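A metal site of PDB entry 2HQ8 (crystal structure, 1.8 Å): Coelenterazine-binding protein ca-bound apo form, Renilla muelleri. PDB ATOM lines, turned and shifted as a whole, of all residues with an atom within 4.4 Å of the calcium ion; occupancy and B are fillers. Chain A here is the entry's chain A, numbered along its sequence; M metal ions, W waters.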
ATOM      1  N   ASP A 112      -6.761 -14.054  18.094  1.00  0.00           N
ATOM      2  CA  ASP A 112      -6.183 -13.387  19.275  1.00  0.00           C
ATOM      3  C   ASP A 112      -6.388 -14.268  20.519  1.00  0.00           C
ATOM      4  O   ASP A 112      -7.336 -14.036  21.292  1.00  0.00           O
ATOM      5  CB  ASP A 112      -6.865 -12.035  19.503  1.00  0.00           C
ATOM      6  CG  ASP A 112      -6.295 -11.288  20.702  1.00  0.00           C
ATOM      7  OD1 ASP A 112      -5.165 -11.602  21.161  1.00  0.00           O
ATOM      8  OD2 ASP A 112      -6.988 -10.376  21.193  1.00  0.00           O
ATOM      9  N   ASP A 114      -4.426 -14.803  23.142  1.00  0.00           N
ATOM     10  CA  ASP A 114      -4.110 -14.271  24.487  1.00  0.00           C
ATOM     11  C   ASP A 114      -4.995 -13.104  24.919  1.00  0.00           C
ATOM     12  O   ASP A 114      -4.833 -12.565  26.008  1.00  0.00           O
ATOM     13  CB  ASP A 114      -2.609 -14.027  24.696  1.00  0.00           C
ATOM     14  CG  ASP A 114      -2.066 -12.885  23.857  1.00  0.00           C
ATOM     15  OD1 ASP A 114      -2.846 -12.135  23.243  1.00  0.00           O
ATOM     16  OD2 ASP A 114      -0.810 -12.782  23.808  1.00  0.00           O
ATOM     17  N   ASP A 116      -5.254  -9.961  24.195  1.00  0.00           N
ATOM     18  CA  ASP A 116      -4.674  -8.656  24.489  1.00  0.00           C
ATOM     19  C   ASP A 116      -5.196  -7.589  23.493  1.00  0.00           C
ATOM     20  O   ASP A 116      -4.874  -6.400  23.629  1.00  0.00           O
ATOM     21  CB  ASP A 116      -3.142  -8.748  24.544  1.00  0.00           C
ATOM     22  CG  ASP A 116      -2.515  -8.839  23.175  1.00  0.00           C
ATOM     23  OD1 ASP A 116      -3.220  -9.196  22.201  1.00  0.00           O
ATOM     24  OD2 ASP A 116      -1.302  -8.533  23.082  1.00  0.00           O
ATOM     25  N   TYR A 118      -4.746  -7.608  20.158  1.00  0.00           N
ATOM     26  CA  TYR A 118      -3.848  -7.518  19.000  1.00  0.00           C
ATOM     27  C   TYR A 118      -3.564  -8.936  18.510  1.00  0.00           C
ATOM     28  O   TYR A 118      -3.596  -9.881  19.291  1.00  0.00           O
ATOM     29  CB  TYR A 118      -2.516  -6.887  19.394  1.00  0.00           C
ATOM     30  CG  TYR A 118      -2.708  -5.454  19.830  1.00  0.00           C
ATOM     31  CD1 TYR A 118      -2.964  -4.455  18.883  1.00  0.00           C
ATOM     32  CD2 TYR A 118      -2.675  -5.121  21.174  1.00  0.00           C
ATOM     33  CE1 TYR A 118      -3.166  -3.128  19.284  1.00  0.00           C
ATOM     34  CE2 TYR A 118      -2.857  -3.801  21.580  1.00  0.00           C
ATOM     35  CZ  TYR A 118      -3.110  -2.834  20.635  1.00  0.00           C
ATOM     36  OH  TYR A 118      -3.298  -1.532  21.058  1.00  0.00           O
ATOM     37  N   VAL A 119      -3.260  -9.042  17.225  1.00  0.00           N
ATOM     38  CA  VAL A 119      -2.813 -10.323  16.653  1.00  0.00           C
ATOM     39  C   VAL A 119      -1.296 -10.283  16.474  1.00  0.00           C
ATOM     40  O   VAL A 119      -0.772  -9.493  15.673  1.00  0.00           O
ATOM     41  CB  VAL A 119      -3.563 -10.666  15.334  1.00  0.00           C
ATOM     42  CG1 VAL A 119      -2.848 -11.785  14.554  1.00  0.00           C
ATOM     43  CG2 VAL A 119      -4.982 -11.047  15.653  1.00  0.00           C
ATOM     44  N   SER A 120      -0.608 -11.098  17.280  1.00  0.00           N
ATOM     45  CA  SER A 120       0.848 -11.201  17.265  1.00  0.00           C
ATOM     46  C   SER A 120       1.372 -12.056  16.104  1.00  0.00           C
ATOM     47  O   SER A 120       0.604 -12.719  15.355  1.00  0.00           O
ATOM     48  CB  SER A 120       1.350 -11.813  18.591  1.00  0.00           C
ATOM     49  OG  SER A 120       1.001 -13.185  18.662  1.00  0.00           O
ATOM     50  N   GLU A 123       0.487 -15.676  16.946  1.00  0.00           N
ATOM     51  CA  GLU A 123      -0.954 -15.928  16.760  1.00  0.00           C
ATOM     52  C   GLU A 123      -1.316 -16.054  15.267  1.00  0.00           C
ATOM     53  O   GLU A 123      -2.071 -16.966  14.860  1.00  0.00           O
ATOM     54  CB  GLU A 123      -1.822 -14.858  17.467  1.00  0.00           C
ATOM     55  CG  GLU A 123      -1.853 -14.993  19.016  1.00  0.00           C
ATOM     56  CD  GLU A 123      -2.346 -13.725  19.729  1.00  0.00           C
ATOM     57  OE1 GLU A 123      -2.370 -12.650  19.081  1.00  0.00           O
ATOM     58  OE2 GLU A 123      -2.732 -13.801  20.913  1.00  0.00           O
HETATM   59 CA    CA M   1      -3.008 -11.325  20.930  1.00  0.00          CA
HETATM   60  O   HOH W   1      -0.378 -10.815  21.313  1.00  0.00           O
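N of Glu 123 is in hydrogen-bond range of OG of Ser 120.
OD1 of Asp 112 is bound to the calcium ion (2.2 Å).
O of Tyr 118 binds the calcium ion (2.3 Å).
OE1 of Glu 123 binds the calcium ion.
The calcium ion is bound by OD1 of Asp 114, 2.5 Å away.
OD1 of Asp 116 binds the calcium ion, at 2.5 Å.
The calcium ion is bound by the side-chain carboxylate (OE2) of Glu 123 (2.5 Å).
Water W1 binds the calcium ion (2.7 Å).
The calcium ion has seven donor atoms within binding distance.
Water W1 lies within hydrogen-bond range of OD2 of Asp 116 (3.0 Å) and OD2 of Asp 114 (3.2 Å).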
